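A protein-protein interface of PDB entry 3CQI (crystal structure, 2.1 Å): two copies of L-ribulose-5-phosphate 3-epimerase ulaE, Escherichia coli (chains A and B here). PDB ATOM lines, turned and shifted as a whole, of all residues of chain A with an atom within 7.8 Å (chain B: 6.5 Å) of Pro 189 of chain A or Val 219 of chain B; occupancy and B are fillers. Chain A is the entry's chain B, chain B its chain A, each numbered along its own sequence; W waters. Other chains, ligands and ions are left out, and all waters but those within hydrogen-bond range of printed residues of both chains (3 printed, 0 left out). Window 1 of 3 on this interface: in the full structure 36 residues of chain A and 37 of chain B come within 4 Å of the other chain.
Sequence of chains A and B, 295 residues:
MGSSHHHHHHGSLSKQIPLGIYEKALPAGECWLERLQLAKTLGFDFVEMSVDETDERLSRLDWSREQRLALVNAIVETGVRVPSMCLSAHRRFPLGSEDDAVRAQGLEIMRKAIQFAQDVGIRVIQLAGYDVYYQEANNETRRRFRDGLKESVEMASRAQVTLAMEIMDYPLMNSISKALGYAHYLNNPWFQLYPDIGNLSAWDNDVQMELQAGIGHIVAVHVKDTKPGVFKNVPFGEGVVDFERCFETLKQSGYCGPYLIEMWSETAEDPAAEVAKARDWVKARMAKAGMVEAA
Water W3 lies within hydrogen-bond range of the backbone carbonyl oxygen of Ser 157 of chain A (2.7 Å), the indole nitrogen of Trp 190 of chain A (2.7 Å) and the backbone carbonyl oxygen of Val 219 of chain B (2.8 Å). Water W1 lies within hydrogen-bond range of NE2 of Gln 192 of chain A and NE2 of Gln 192 of chain B.
Pro 189 of chain A touches Gln 192 of chain B, and with the chains exchanged Gln 192 of chain A touches Pro 189 of chain B. Pro 189 of chain A touches Val 219 of chain B, and with the chains exchanged Val 219 of chain A touches Pro 189 of chain B. Gln 192 of chain B touches its own counterpart, Gln 192 of chain A. Positions printed for both chains: 162, 163, 189, 192, 217 and 219.
Pro 189 of chain A touches four residues of chain B. Printed residues of chain A within 4 Å of Gln 192 of chain B: Pro 189 (3.6 Å) and Gln 192 (3.9 Å). His 217 of chain B touches none of the printed residues of chain A. Val 219 of chain B touches just these residues of chain A: Gln 160, Pro 189 and Trp 190. Printed residues of chain A within 4 Å of Pro 258 of chain B: Ser 157 (3.5 Å) and Gln 160 (3.5 Å).
Printed residues of chain A that touch a printed residue of chain B: Ser 157, Gln 160, Asn 187, Asn 188, Pro 189, Trp 190, Gln 192 and Val 219. Hydrophobic or aromatic side chains of chain B within 4 Å of the printed part of chain A: Val 124, Pro 189, Val 219, Ala 220 and Pro 258. Among the printed residues, 19 pairs touch across the chains. Among the printed residues, no Asp or Glu carboxylate lies within 4 Å of a Lys or Arg side-chain nitrogen of the other chain.
The backbone carbonyl oxygen (O) of Ile 215 of chain B sits at hydrogen-bond distance from the side-chain amide nitrogen (ND2) of Asn 187 of chain A, 3.4 Å away. O of Val 219 of chain B sits at hydrogen-bond distance from NE2 of Gln 160 of chain A (2.9 Å). The backbone carbonyl oxygen (O) of Gly 216 of chain B sits close to the backbone nitrogen (N) of Pro 189 of chain A (3.3 Å).
The side-chain hydroxyl (OH) of Tyr 255 of chain B sits at hydrogen-bond distance from the backbone carbonyl oxygen (O) of Pro 258 of chain B (2.7 Å). O of Val 153 of chain A is in hydrogen-bond range of OG of Ser 157 of chain A, 2.8 Å away. The side-chain amide oxygen of Gln 192 of chain A sits at hydrogen-bond distance from a ring nitrogen (ND1) of His 217 of chain A, 2.7 Å away.
Among the printed residues, merely in contact across the chains: Asn 187 of chain A with Gly 216 of chain B (3.3 Å), Ser 157 of chain A with Gly 257 of chain B (3.4 Å), Gln 160 of chain A with Pro 258 of chain B (3.5 Å), Trp 190 of chain A with Thr 162 of chain B (3.5 Å), Ser 157 of chain A with Pro 258 of chain B (3.5 Å), Gln 160 of chain A with Ala 220 of chain B (3.6 Å), Pro 189 of chain A with Ile 218 of chain B (3.6 Å), Val 219 of chain A with Pro 189 of chain B (3.6 Å), Trp 190 of chain A with Val 124 of chain B (3.6 Å), Pro 189 of chain A with Gln 192 of chain B (3.6 Å), Trp 190 of chain A with Val 219 of chain B (3.7 Å), Pro 189 of chain A with Val 219 of chain B (3.7 Å), Gln 192 of chain A with Pro 189 of chain B (3.8 Å), Gln 192 of chain A with Gln 192 of chain B (3.9 Å), Gln 160 of chain A with Val 124 of chain B (3.9 Å) and Asn 188 of chain A with Gly 216 of chain B (3.9 Å).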
ATOM      1  N   VAL A 153      21.494  18.441  -7.238  1.00  0.00           N
ATOM      2  CA  VAL A 153      20.647  17.323  -7.647  1.00  0.00           C
ATOM      3  C   VAL A 153      21.439  15.996  -7.730  1.00  0.00           C
ATOM      4  O   VAL A 153      20.886  14.931  -7.471  1.00  0.00           O
ATOM      5  CB  VAL A 153      19.863  17.667  -8.970  1.00  0.00           C
ATOM      6  CG1 VAL A 153      19.288  16.464  -9.583  1.00  0.00           C
ATOM      7  CG2 VAL A 153      18.742  18.665  -8.679  1.00  0.00           C
ATOM      8  N   ALA A 156      21.685  14.940  -4.165  1.00  0.00           N
ATOM      9  CA  ALA A 156      20.380  14.413  -3.769  1.00  0.00           C
ATOM     10  C   ALA A 156      20.101  13.036  -4.370  1.00  0.00           C
ATOM     11  O   ALA A 156      19.398  12.243  -3.763  1.00  0.00           O
ATOM     12  CB  ALA A 156      19.271  15.371  -4.138  1.00  0.00           C
ATOM     13  N   SER A 157      20.649  12.763  -5.556  1.00  0.00           N
ATOM     14  CA  SER A 157      20.488  11.459  -6.198  1.00  0.00           C
ATOM     15  C   SER A 157      21.196  10.348  -5.444  1.00  0.00           C
ATOM     16  O   SER A 157      20.728   9.206  -5.438  1.00  0.00           O
ATOM     17  CB  SER A 157      20.978  11.485  -7.645  1.00  0.00           C
ATOM     18  OG  SER A 157      20.167  12.360  -8.401  1.00  0.00           O
ATOM     19  N   ARG A 158      22.337  10.673  -4.853  1.00  0.00           N
ATOM     20  CA  ARG A 158      23.117   9.693  -4.091  1.00  0.00           C
ATOM     21  C   ARG A 158      22.452   9.394  -2.758  1.00  0.00           C
ATOM     22  O   ARG A 158      22.420   8.232  -2.307  1.00  0.00           O
ATOM     23  CB  ARG A 158      24.545  10.195  -3.852  1.00  0.00           C
ATOM     24  CG  ARG A 158      25.340  10.290  -5.124  1.00  0.00           C
ATOM     25  CD  ARG A 158      26.786  10.551  -4.847  1.00  0.00           C
ATOM     26  NE  ARG A 158      27.018  11.924  -4.429  1.00  0.00           N
ATOM     27  CZ  ARG A 158      27.320  12.928  -5.252  1.00  0.00           C
ATOM     28  NH1 ARG A 158      27.406  12.727  -6.562  1.00  0.00           N
ATOM     29  NH2 ARG A 158      27.524  14.146  -4.757  1.00  0.00           N
ATOM     30  N   ALA A 159      21.915  10.454  -2.153  1.00  0.00           N
ATOM     31  CA  ALA A 159      21.288  10.385  -0.850  1.00  0.00           C
ATOM     32  C   ALA A 159      19.824   9.952  -0.944  1.00  0.00           C
ATOM     33  O   ALA A 159      19.231   9.493   0.053  1.00  0.00           O
ATOM     34  CB  ALA A 159      21.400  11.733  -0.154  1.00  0.00           C
ATOM     35  N   GLN A 160      19.257  10.085  -2.142  1.00  0.00           N
ATOM     36  CA  GLN A 160      17.833   9.794  -2.403  1.00  0.00           C
ATOM     37  C   GLN A 160      16.917  10.706  -1.567  1.00  0.00           C
ATOM     38  O   GLN A 160      16.002  10.247  -0.868  1.00  0.00           O
ATOM     39  CB  GLN A 160      17.520   8.293  -2.230  1.00  0.00           C
ATOM     40  CG  GLN A 160      18.219   7.367  -3.267  1.00  0.00           C
ATOM     41  CD  GLN A 160      18.084   5.871  -2.935  1.00  0.00           C
ATOM     42  OE1 GLN A 160      18.411   5.431  -1.826  1.00  0.00           O
ATOM     43  NE2 GLN A 160      17.629   5.085  -3.904  1.00  0.00           N
ATOM     44  N   VAL A 161      17.196  12.000  -1.628  1.00  0.00           N
ATOM     45  CA  VAL A 161      16.442  13.005  -0.889  1.00  0.00           C
ATOM     46  C   VAL A 161      15.851  13.931  -1.948  1.00  0.00           C
ATOM     47  O   VAL A 161      16.559  14.336  -2.866  1.00  0.00           O
ATOM     48  CB  VAL A 161      17.366  13.809   0.063  1.00  0.00           C
ATOM     49  CG1 VAL A 161      16.654  15.098   0.614  1.00  0.00           C
ATOM     50  CG2 VAL A 161      17.869  12.921   1.201  1.00  0.00           C
ATOM     51  N   THR A 162      14.554  14.222  -1.834  1.00  0.00           N
ATOM     52  CA  THR A 162      13.850  15.100  -2.771  1.00  0.00           C
ATOM     53  C   THR A 162      14.195  16.585  -2.557  1.00  0.00           C
ATOM     54  O   THR A 162      14.106  17.085  -1.435  1.00  0.00           O
ATOM     55  CB  THR A 162      12.305  14.903  -2.670  1.00  0.00           C
ATOM     56  OG1 THR A 162      11.973  13.540  -2.980  1.00  0.00           O
ATOM     57  CG2 THR A 162      11.565  15.832  -3.640  1.00  0.00           C
ATOM     58  N   LEU A 163      14.614  17.264  -3.636  1.00  0.00           N
ATOM     59  CA  LEU A 163      14.751  18.726  -3.662  1.00  0.00           C
ATOM     60  C   LEU A 163      13.577  19.302  -4.454  1.00  0.00           C
ATOM     61  O   LEU A 163      13.363  18.931  -5.607  1.00  0.00           O
ATOM     62  CB  LEU A 163      16.081  19.149  -4.318  1.00  0.00           C
ATOM     63  CG  LEU A 163      17.390  18.545  -3.783  1.00  0.00           C
ATOM     64  CD1 LEU A 163      18.621  19.162  -4.466  1.00  0.00           C
ATOM     65  CD2 LEU A 163      17.490  18.726  -2.279  1.00  0.00           C
ATOM     66  N   ALA A 183      13.256  21.613 -14.467  1.00  0.00           N
ATOM     67  CA  ALA A 183      12.979  20.170 -14.379  1.00  0.00           C
ATOM     68  C   ALA A 183      13.317  19.444 -15.659  1.00  0.00           C
ATOM     69  O   ALA A 183      13.874  18.344 -15.600  1.00  0.00           O
ATOM     70  CB  ALA A 183      11.514  19.908 -13.991  1.00  0.00           C
ATOM     71  N   LEU A 186      17.185  19.334 -15.963  1.00  0.00           N
ATOM     72  CA  LEU A 186      17.831  18.425 -15.028  1.00  0.00           C
ATOM     73  C   LEU A 186      17.463  16.956 -15.248  1.00  0.00           C
ATOM     74  O   LEU A 186      18.311  16.088 -15.022  1.00  0.00           O
ATOM     75  CB  LEU A 186      17.534  18.845 -13.590  1.00  0.00           C
ATOM     76  CG  LEU A 186      18.088  20.219 -13.201  1.00  0.00           C
ATOM     77  CD1 LEU A 186      17.301  20.809 -12.042  1.00  0.00           C
ATOM     78  CD2 LEU A 186      19.549  20.109 -12.846  1.00  0.00           C
ATOM     79  N   ASN A 187      16.222  16.708 -15.704  1.00  0.00           N
ATOM     80  CA  ASN A 187      15.685  15.363 -16.000  1.00  0.00           C
ATOM     81  C   ASN A 187      16.101  14.346 -14.936  1.00  0.00           C
ATOM     82  O   ASN A 187      16.724  13.340 -15.226  1.00  0.00           O
ATOM     83  CB  ASN A 187      16.090  14.889 -17.407  1.00  0.00           C
ATOM     84  CG  ASN A 187      15.371  13.621 -17.829  1.00  0.00           C
ATOM     85  OD1 ASN A 187      14.205  13.410 -17.493  1.00  0.00           O
ATOM     86  ND2 ASN A 187      16.059  12.772 -18.571  1.00  0.00           N
ATOM     87  N   ASN A 188      15.755  14.653 -13.696  1.00  0.00           N
ATOM     88  CA  ASN A 188      16.161  13.879 -12.545  1.00  0.00           C
ATOM     89  C   ASN A 188      14.976  13.706 -11.610  1.00  0.00           C
ATOM     90  O   ASN A 188      14.314  14.698 -11.269  1.00  0.00           O
ATOM     91  CB  ASN A 188      17.284  14.613 -11.812  1.00  0.00           C
ATOM     92  CG  ASN A 188      17.848  13.805 -10.640  1.00  0.00           C
ATOM     93  OD1 ASN A 188      17.228  13.704  -9.600  1.00  0.00           O
ATOM     94  ND2 ASN A 188      19.023  13.237 -10.822  1.00  0.00           N
ATOM     95  N   PRO A 189      14.731  12.457 -11.157  1.00  0.00           N
ATOM     96  CA  PRO A 189      13.575  12.137 -10.312  1.00  0.00           C
ATOM     97  C   PRO A 189      13.589  12.856  -8.960  1.00  0.00           C
ATOM     98  O   PRO A 189      12.548  13.012  -8.341  1.00  0.00           O
ATOM     99  CB  PRO A 189      13.680  10.611 -10.109  1.00  0.00           C
ATOM    100  CG  PRO A 189      15.078  10.268 -10.390  1.00  0.00           C
ATOM    101  CD  PRO A 189      15.560  11.262 -11.427  1.00  0.00           C
ATOM    102  N   TRP A 190      14.755  13.323  -8.528  1.00  0.00           N
ATOM    103  CA  TRP A 190      14.861  13.983  -7.226  1.00  0.00           C
ATOM    104  C   TRP A 190      14.692  15.499  -7.276  1.00  0.00           C
ATOM    105  O   TRP A 190      14.851  16.155  -6.258  1.00  0.00           O
ATOM    106  CB  TRP A 190      16.159  13.566  -6.524  1.00  0.00           C
ATOM    107  CG  TRP A 190      16.211  12.082  -6.303  1.00  0.00           C
ATOM    108  CD1 TRP A 190      16.990  11.183  -6.967  1.00  0.00           C
ATOM    109  CD2 TRP A 190      15.420  11.328  -5.373  1.00  0.00           C
ATOM    110  NE1 TRP A 190      16.758   9.912  -6.494  1.00  0.00           N
ATOM    111  CE2 TRP A 190      15.793   9.973  -5.514  1.00  0.00           C
ATOM    112  CE3 TRP A 190      14.445  11.669  -4.427  1.00  0.00           C
ATOM    113  CZ2 TRP A 190      15.212   8.949  -4.754  1.00  0.00           C
ATOM    114  CZ3 TRP A 190      13.872  10.648  -3.651  1.00  0.00           C
ATOM    115  CH2 TRP A 190      14.254   9.303  -3.829  1.00  0.00           C
ATOM    116  N   PHE A 191      14.380  16.050  -8.454  1.00  0.00           N
ATOM    117  CA  PHE A 191      14.028  17.459  -8.579  1.00  0.00           C
ATOM    118  C   PHE A 191      12.533  17.548  -8.873  1.00  0.00           C
ATOM    119  O   PHE A 191      12.050  16.993  -9.876  1.00  0.00           O
ATOM    120  CB  PHE A 191      14.823  18.162  -9.701  1.00  0.00           C
ATOM    121  CG  PHE A 191      14.525  19.641  -9.821  1.00  0.00           C
ATOM    122  CD1 PHE A 191      15.154  20.567  -8.978  1.00  0.00           C
ATOM    123  CD2 PHE A 191      13.612  20.111 -10.776  1.00  0.00           C
ATOM    124  CE1 PHE A 191      14.881  21.931  -9.084  1.00  0.00           C
ATOM    125  CE2 PHE A 191      13.333  21.496 -10.885  1.00  0.00           C
ATOM    126  CZ  PHE A 191      13.968  22.396 -10.038  1.00  0.00           C
ATOM    127  N   GLN A 192      11.817  18.236  -7.985  1.00  0.00           N
ATOM    128  CA  GLN A 192      10.363  18.377  -8.065  1.00  0.00           C
ATOM    129  C   GLN A 192       9.946  19.818  -7.741  1.00  0.00           C
ATOM    130  O   GLN A 192      10.795  20.717  -7.663  1.00  0.00           O
ATOM    131  CB  GLN A 192       9.669  17.368  -7.117  1.00  0.00           C
ATOM    132  CG  GLN A 192      10.029  15.853  -7.378  1.00  0.00           C
ATOM    133  CD  GLN A 192       9.645  15.377  -8.779  1.00  0.00           C
ATOM    134  OE1 GLN A 192       8.909  16.047  -9.484  1.00  0.00           O
ATOM    135  NE2 GLN A 192      10.153  14.215  -9.183  1.00  0.00           N
ATOM    136  N   HIS A 217       4.641  16.754 -10.836  1.00  0.00           N
ATOM    137  CA  HIS A 217       5.822  17.245 -10.129  1.00  0.00           C
ATOM    138  C   HIS A 217       5.563  17.927  -8.776  1.00  0.00           C
ATOM    139  O   HIS A 217       6.493  18.154  -8.003  1.00  0.00           O
ATOM    140  CB  HIS A 217       6.641  18.170 -11.046  1.00  0.00           C
ATOM    141  CG  HIS A 217       7.228  17.456 -12.226  1.00  0.00           C
ATOM    142  ND1 HIS A 217       8.202  16.488 -12.098  1.00  0.00           N
ATOM    143  CD2 HIS A 217       6.950  17.533 -13.548  1.00  0.00           C
ATOM    144  CE1 HIS A 217       8.516  16.017 -13.293  1.00  0.00           C
ATOM    145  NE2 HIS A 217       7.777  16.641 -14.190  1.00  0.00           N
ATOM    146  N   VAL A 219       4.896  18.204  -5.118  1.00  0.00           N
ATOM    147  CA  VAL A 219       5.071  17.279  -3.992  1.00  0.00           C
ATOM    148  C   VAL A 219       4.562  17.838  -2.663  1.00  0.00           C
ATOM    149  O   VAL A 219       4.378  17.087  -1.697  1.00  0.00           O
ATOM    150  CB  VAL A 219       6.547  16.837  -3.791  1.00  0.00           C
ATOM    151  CG1 VAL A 219       7.021  15.922  -4.948  1.00  0.00           C
ATOM    152  CG2 VAL A 219       7.492  18.039  -3.573  1.00  0.00           C
ATOM    153  N   VAL B 124      13.229   5.078  -0.049  1.00  0.00           N
ATOM    154  CA  VAL B 124      12.590   4.448  -1.196  1.00  0.00           C
ATOM    155  C   VAL B 124      12.057   3.065  -0.827  1.00  0.00           C
ATOM    156  O   VAL B 124      12.786   2.245  -0.294  1.00  0.00           O
ATOM    157  CB  VAL B 124      13.575   4.374  -2.436  1.00  0.00           C
ATOM    158  CG1 VAL B 124      13.028   3.481  -3.544  1.00  0.00           C
ATOM    159  CG2 VAL B 124      13.875   5.783  -3.003  1.00  0.00           C
ATOM    160  N   THR B 162       8.861   7.887  -1.559  1.00  0.00           N
ATOM    161  CA  THR B 162       9.017   7.365  -2.916  1.00  0.00           C
ATOM    162  C   THR B 162       8.735   5.861  -2.976  1.00  0.00           C
ATOM    163  O   THR B 162       9.296   5.075  -2.203  1.00  0.00           O
ATOM    164  CB  THR B 162      10.463   7.618  -3.473  1.00  0.00           C
ATOM    165  OG1 THR B 162      10.758   9.019  -3.436  1.00  0.00           O
ATOM    166  CG2 THR B 162      10.588   7.131  -4.924  1.00  0.00           C
ATOM    167  N   LEU B 163       7.870   5.475  -3.911  1.00  0.00           N
ATOM    168  CA  LEU B 163       7.691   4.070  -4.280  1.00  0.00           C
ATOM    169  C   LEU B 163       8.335   3.895  -5.646  1.00  0.00           C
ATOM    170  O   LEU B 163       8.039   4.662  -6.568  1.00  0.00           O
ATOM    171  CB  LEU B 163       6.198   3.695  -4.362  1.00  0.00           C
ATOM    172  CG  LEU B 163       5.278   4.066  -3.191  1.00  0.00           C
ATOM    173  CD1 LEU B 163       3.820   3.718  -3.481  1.00  0.00           C
ATOM    174  CD2 LEU B 163       5.754   3.431  -1.841  1.00  0.00           C
ATOM    175  N   ALA B 164       9.200   2.893  -5.777  1.00  0.00           N
ATOM    176  CA  ALA B 164       9.939   2.676  -7.007  1.00  0.00           C
ATOM    177  C   ALA B 164       9.697   1.264  -7.486  1.00  0.00           C
ATOM    178  O   ALA B 164       9.963   0.283  -6.773  1.00  0.00           O
ATOM    179  CB  ALA B 164      11.435   2.932  -6.794  1.00  0.00           C
ATOM    180  N   PRO B 189       4.802  12.267  -8.753  1.00  0.00           N
ATOM    181  CA  PRO B 189       6.233  12.370  -8.437  1.00  0.00           C
ATOM    182  C   PRO B 189       6.768  11.283  -7.485  1.00  0.00           C
ATOM    183  O   PRO B 189       7.981  11.040  -7.433  1.00  0.00           O
ATOM    184  CB  PRO B 189       6.367  13.762  -7.803  1.00  0.00           C
ATOM    185  CG  PRO B 189       4.964  14.169  -7.373  1.00  0.00           C
ATOM    186  CD  PRO B 189       4.036  13.462  -8.319  1.00  0.00           C
ATOM    187  N   GLN B 192       8.338   6.027  -9.033  1.00  0.00           N
ATOM    188  CA  GLN B 192       9.579   6.029  -9.802  1.00  0.00           C
ATOM    189  C   GLN B 192      10.008   4.609 -10.198  1.00  0.00           C
ATOM    190  O   GLN B 192       9.232   3.656 -10.048  1.00  0.00           O
ATOM    191  CB  GLN B 192      10.704   6.791  -9.067  1.00  0.00           C
ATOM    192  CG  GLN B 192      10.424   8.281  -8.724  1.00  0.00           C
ATOM    193  CD  GLN B 192      10.252   9.190  -9.938  1.00  0.00           C
ATOM    194  OE1 GLN B 192      10.634   8.850 -11.053  1.00  0.00           O
ATOM    195  NE2 GLN B 192       9.675  10.363  -9.711  1.00  0.00           N
ATOM    196  N   LEU B 193      11.228   4.485 -10.721  1.00  0.00           N
ATOM    197  CA  LEU B 193      11.739   3.221 -11.262  1.00  0.00           C
ATOM    198  C   LEU B 193      12.960   2.698 -10.521  1.00  0.00           C
ATOM    199  O   LEU B 193      13.882   3.438 -10.191  1.00  0.00           O
ATOM    200  CB  LEU B 193      12.106   3.371 -12.739  1.00  0.00           C
ATOM    201  CG  LEU B 193      11.021   3.072 -13.783  1.00  0.00           C
ATOM    202  CD1 LEU B 193       9.696   3.720 -13.491  1.00  0.00           C
ATOM    203  CD2 LEU B 193      11.522   3.487 -15.156  1.00  0.00           C
ATOM    204  N   TYR B 194      12.968   1.397 -10.292  1.00  0.00           N
ATOM    205  CA  TYR B 194      14.100   0.766  -9.641  1.00  0.00           C
ATOM    206  C   TYR B 194      14.468  -0.442 -10.502  1.00  0.00           C
ATOM    207  O   TYR B 194      14.132  -1.569 -10.146  1.00  0.00           O
ATOM    208  CB  TYR B 194      13.682   0.332  -8.237  1.00  0.00           C
ATOM    209  CG  TYR B 194      14.792  -0.002  -7.253  1.00  0.00           C
ATOM    210  CD1 TYR B 194      14.603   0.212  -5.890  1.00  0.00           C
ATOM    211  CD2 TYR B 194      16.009  -0.567  -7.678  1.00  0.00           C
ATOM    212  CE1 TYR B 194      15.595  -0.117  -4.962  1.00  0.00           C
ATOM    213  CE2 TYR B 194      17.015  -0.893  -6.761  1.00  0.00           C
ATOM    214  CZ  TYR B 194      16.789  -0.666  -5.398  1.00  0.00           C
ATOM    215  OH  TYR B 194      17.767  -0.965  -4.483  1.00  0.00           O
ATOM    216  N   PRO B 195      15.158  -0.215 -11.639  1.00  0.00           N
ATOM    217  CA  PRO B 195      15.489  -1.372 -12.465  1.00  0.00           C
ATOM    218  C   PRO B 195      16.451  -2.366 -11.819  1.00  0.00           C
ATOM    219  O   PRO B 195      17.345  -1.995 -11.070  1.00  0.00           O
ATOM    220  CB  PRO B 195      16.105  -0.753 -13.727  1.00  0.00           C
ATOM    221  CG  PRO B 195      16.543   0.596 -13.345  1.00  0.00           C
ATOM    222  CD  PRO B 195      15.616   1.051 -12.245  1.00  0.00           C
ATOM    223  N   ILE B 215      15.986   6.919 -17.712  1.00  0.00           N
ATOM    224  CA  ILE B 215      16.675   8.064 -17.130  1.00  0.00           C
ATOM    225  C   ILE B 215      15.701   9.235 -16.988  1.00  0.00           C
ATOM    226  O   ILE B 215      15.004   9.644 -17.943  1.00  0.00           O
ATOM    227  CB  ILE B 215      17.980   8.431 -17.908  1.00  0.00           C
ATOM    228  CG1 ILE B 215      18.976   7.279 -17.804  1.00  0.00           C
ATOM    229  CG2 ILE B 215      18.639   9.701 -17.362  1.00  0.00           C
ATOM    230  CD1 ILE B 215      19.853   7.299 -16.537  1.00  0.00           C
ATOM    231  N   GLY B 216      15.622   9.730 -15.766  1.00  0.00           N
ATOM    232  CA  GLY B 216      14.639  10.737 -15.424  1.00  0.00           C
ATOM    233  C   GLY B 216      13.727  10.130 -14.384  1.00  0.00           C
ATOM    234  O   GLY B 216      13.129  10.849 -13.601  1.00  0.00           O
ATOM    235  N   HIS B 217      13.643   8.795 -14.365  1.00  0.00           N
ATOM    236  CA  HIS B 217      12.807   8.107 -13.382  1.00  0.00           C
ATOM    237  C   HIS B 217      13.555   7.068 -12.547  1.00  0.00           C
ATOM    238  O   HIS B 217      13.011   6.548 -11.591  1.00  0.00           O
ATOM    239  CB  HIS B 217      11.592   7.477 -14.073  1.00  0.00           C
ATOM    240  CG  HIS B 217      10.682   8.488 -14.687  1.00  0.00           C
ATOM    241  ND1 HIS B 217       9.805   9.250 -13.941  1.00  0.00           N
ATOM    242  CD2 HIS B 217      10.546   8.900 -15.969  1.00  0.00           C
ATOM    243  CE1 HIS B 217       9.164  10.081 -14.743  1.00  0.00           C
ATOM    244  NE2 HIS B 217       9.592   9.884 -15.978  1.00  0.00           N
ATOM    245  N   ILE B 218      14.790   6.759 -12.920  1.00  0.00           N
ATOM    246  CA  ILE B 218      15.578   5.741 -12.205  1.00  0.00           C
ATOM    247  C   ILE B 218      16.148   6.294 -10.895  1.00  0.00           C
ATOM    248  O   ILE B 218      16.949   7.242 -10.906  1.00  0.00           O
ATOM    249  CB  ILE B 218      16.722   5.173 -13.113  1.00  0.00           C
ATOM    250  CG1 ILE B 218      16.116   4.400 -14.302  1.00  0.00           C
ATOM    251  CG2 ILE B 218      17.646   4.265 -12.310  1.00  0.00           C
ATOM    252  CD1 ILE B 218      17.083   4.148 -15.465  1.00  0.00           C
ATOM    253  N   VAL B 219      15.769   5.695  -9.769  1.00  0.00           N
ATOM    254  CA  VAL B 219      16.199   6.200  -8.441  1.00  0.00           C
ATOM    255  C   VAL B 219      17.220   5.289  -7.733  1.00  0.00           C
ATOM    256  O   VAL B 219      17.880   5.703  -6.754  1.00  0.00           O
ATOM    257  CB  VAL B 219      14.981   6.466  -7.478  1.00  0.00           C
ATOM    258  CG1 VAL B 219      14.076   7.600  -8.006  1.00  0.00           C
ATOM    259  CG2 VAL B 219      14.172   5.195  -7.250  1.00  0.00           C
ATOM    260  N   ALA B 220      17.327   4.057  -8.230  1.00  0.00           N
ATOM    261  CA  ALA B 220      18.164   3.021  -7.634  1.00  0.00           C
ATOM    262  C   ALA B 220      18.326   1.915  -8.659  1.00  0.00           C
ATOM    263  O   ALA B 220      17.495   1.777  -9.533  1.00  0.00           O
ATOM    264  CB  ALA B 220      17.507   2.467  -6.356  1.00  0.00           C
ATOM    265  N   VAL B 221      19.389   1.124  -8.548  1.00  0.00           N
ATOM    266  CA  VAL B 221      19.653   0.024  -9.489  1.00  0.00           C
ATOM    267  C   VAL B 221      20.055  -1.219  -8.701  1.00  0.00           C
ATOM    268  O   VAL B 221      20.957  -1.159  -7.860  1.00  0.00           O
ATOM    269  CB  VAL B 221      20.791   0.374 -10.526  1.00  0.00           C
ATOM    270  CG1 VAL B 221      21.083  -0.805 -11.475  1.00  0.00           C
ATOM    271  CG2 VAL B 221      20.463   1.619 -11.334  1.00  0.00           C
ATOM    272  N   TYR B 255      23.193   9.000 -14.857  1.00  0.00           N
ATOM    273  CA  TYR B 255      22.776   8.414 -13.595  1.00  0.00           C
ATOM    274  C   TYR B 255      23.839   8.657 -12.537  1.00  0.00           C
ATOM    275  O   TYR B 255      25.030   8.406 -12.786  1.00  0.00           O
ATOM    276  CB  TYR B 255      22.521   6.909 -13.726  1.00  0.00           C
ATOM    277  CG  TYR B 255      21.983   6.281 -12.451  1.00  0.00           C
ATOM    278  CD1 TYR B 255      20.744   6.656 -11.932  1.00  0.00           C
ATOM    279  CD2 TYR B 255      22.716   5.323 -11.767  1.00  0.00           C
ATOM    280  CE1 TYR B 255      20.250   6.079 -10.752  1.00  0.00           C
ATOM    281  CE2 TYR B 255      22.231   4.742 -10.591  1.00  0.00           C
ATOM    282  CZ  TYR B 255      20.993   5.126 -10.104  1.00  0.00           C
ATOM    283  OH  TYR B 255      20.520   4.541  -8.959  1.00  0.00           O
ATOM    284  N   GLY B 257      22.850   7.886  -9.015  1.00  0.00           N
ATOM    285  CA  GLY B 257      22.269   7.280  -7.809  1.00  0.00           C
ATOM    286  C   GLY B 257      22.984   6.026  -7.313  1.00  0.00           C
ATOM    287  O   GLY B 257      24.044   5.663  -7.837  1.00  0.00           O
ATOM    288  N   PRO B 258      22.407   5.346  -6.300  1.00  0.00           N
ATOM    289  CA  PRO B 258      23.028   4.128  -5.758  1.00  0.00           C
ATOM    290  C   PRO B 258      22.879   2.851  -6.600  1.00  0.00           C
ATOM    291  O   PRO B 258      21.989   2.760  -7.486  1.00  0.00           O
ATOM    292  CB  PRO B 258      22.328   3.931  -4.419  1.00  0.00           C
ATOM    293  CG  PRO B 258      21.044   4.650  -4.530  1.00  0.00           C
ATOM    294  CD  PRO B 258      21.164   5.702  -5.600  1.00  0.00           C
HETATM  295  O   HOH W   1       9.314  12.701 -11.788  1.00  0.00           O
HETATM  296  O   HOH W   2      12.395  11.653 -18.588  1.00  0.00           O
HETATM  297  O   HOH W   3      18.859   8.293  -7.141  1.00  0.00           O
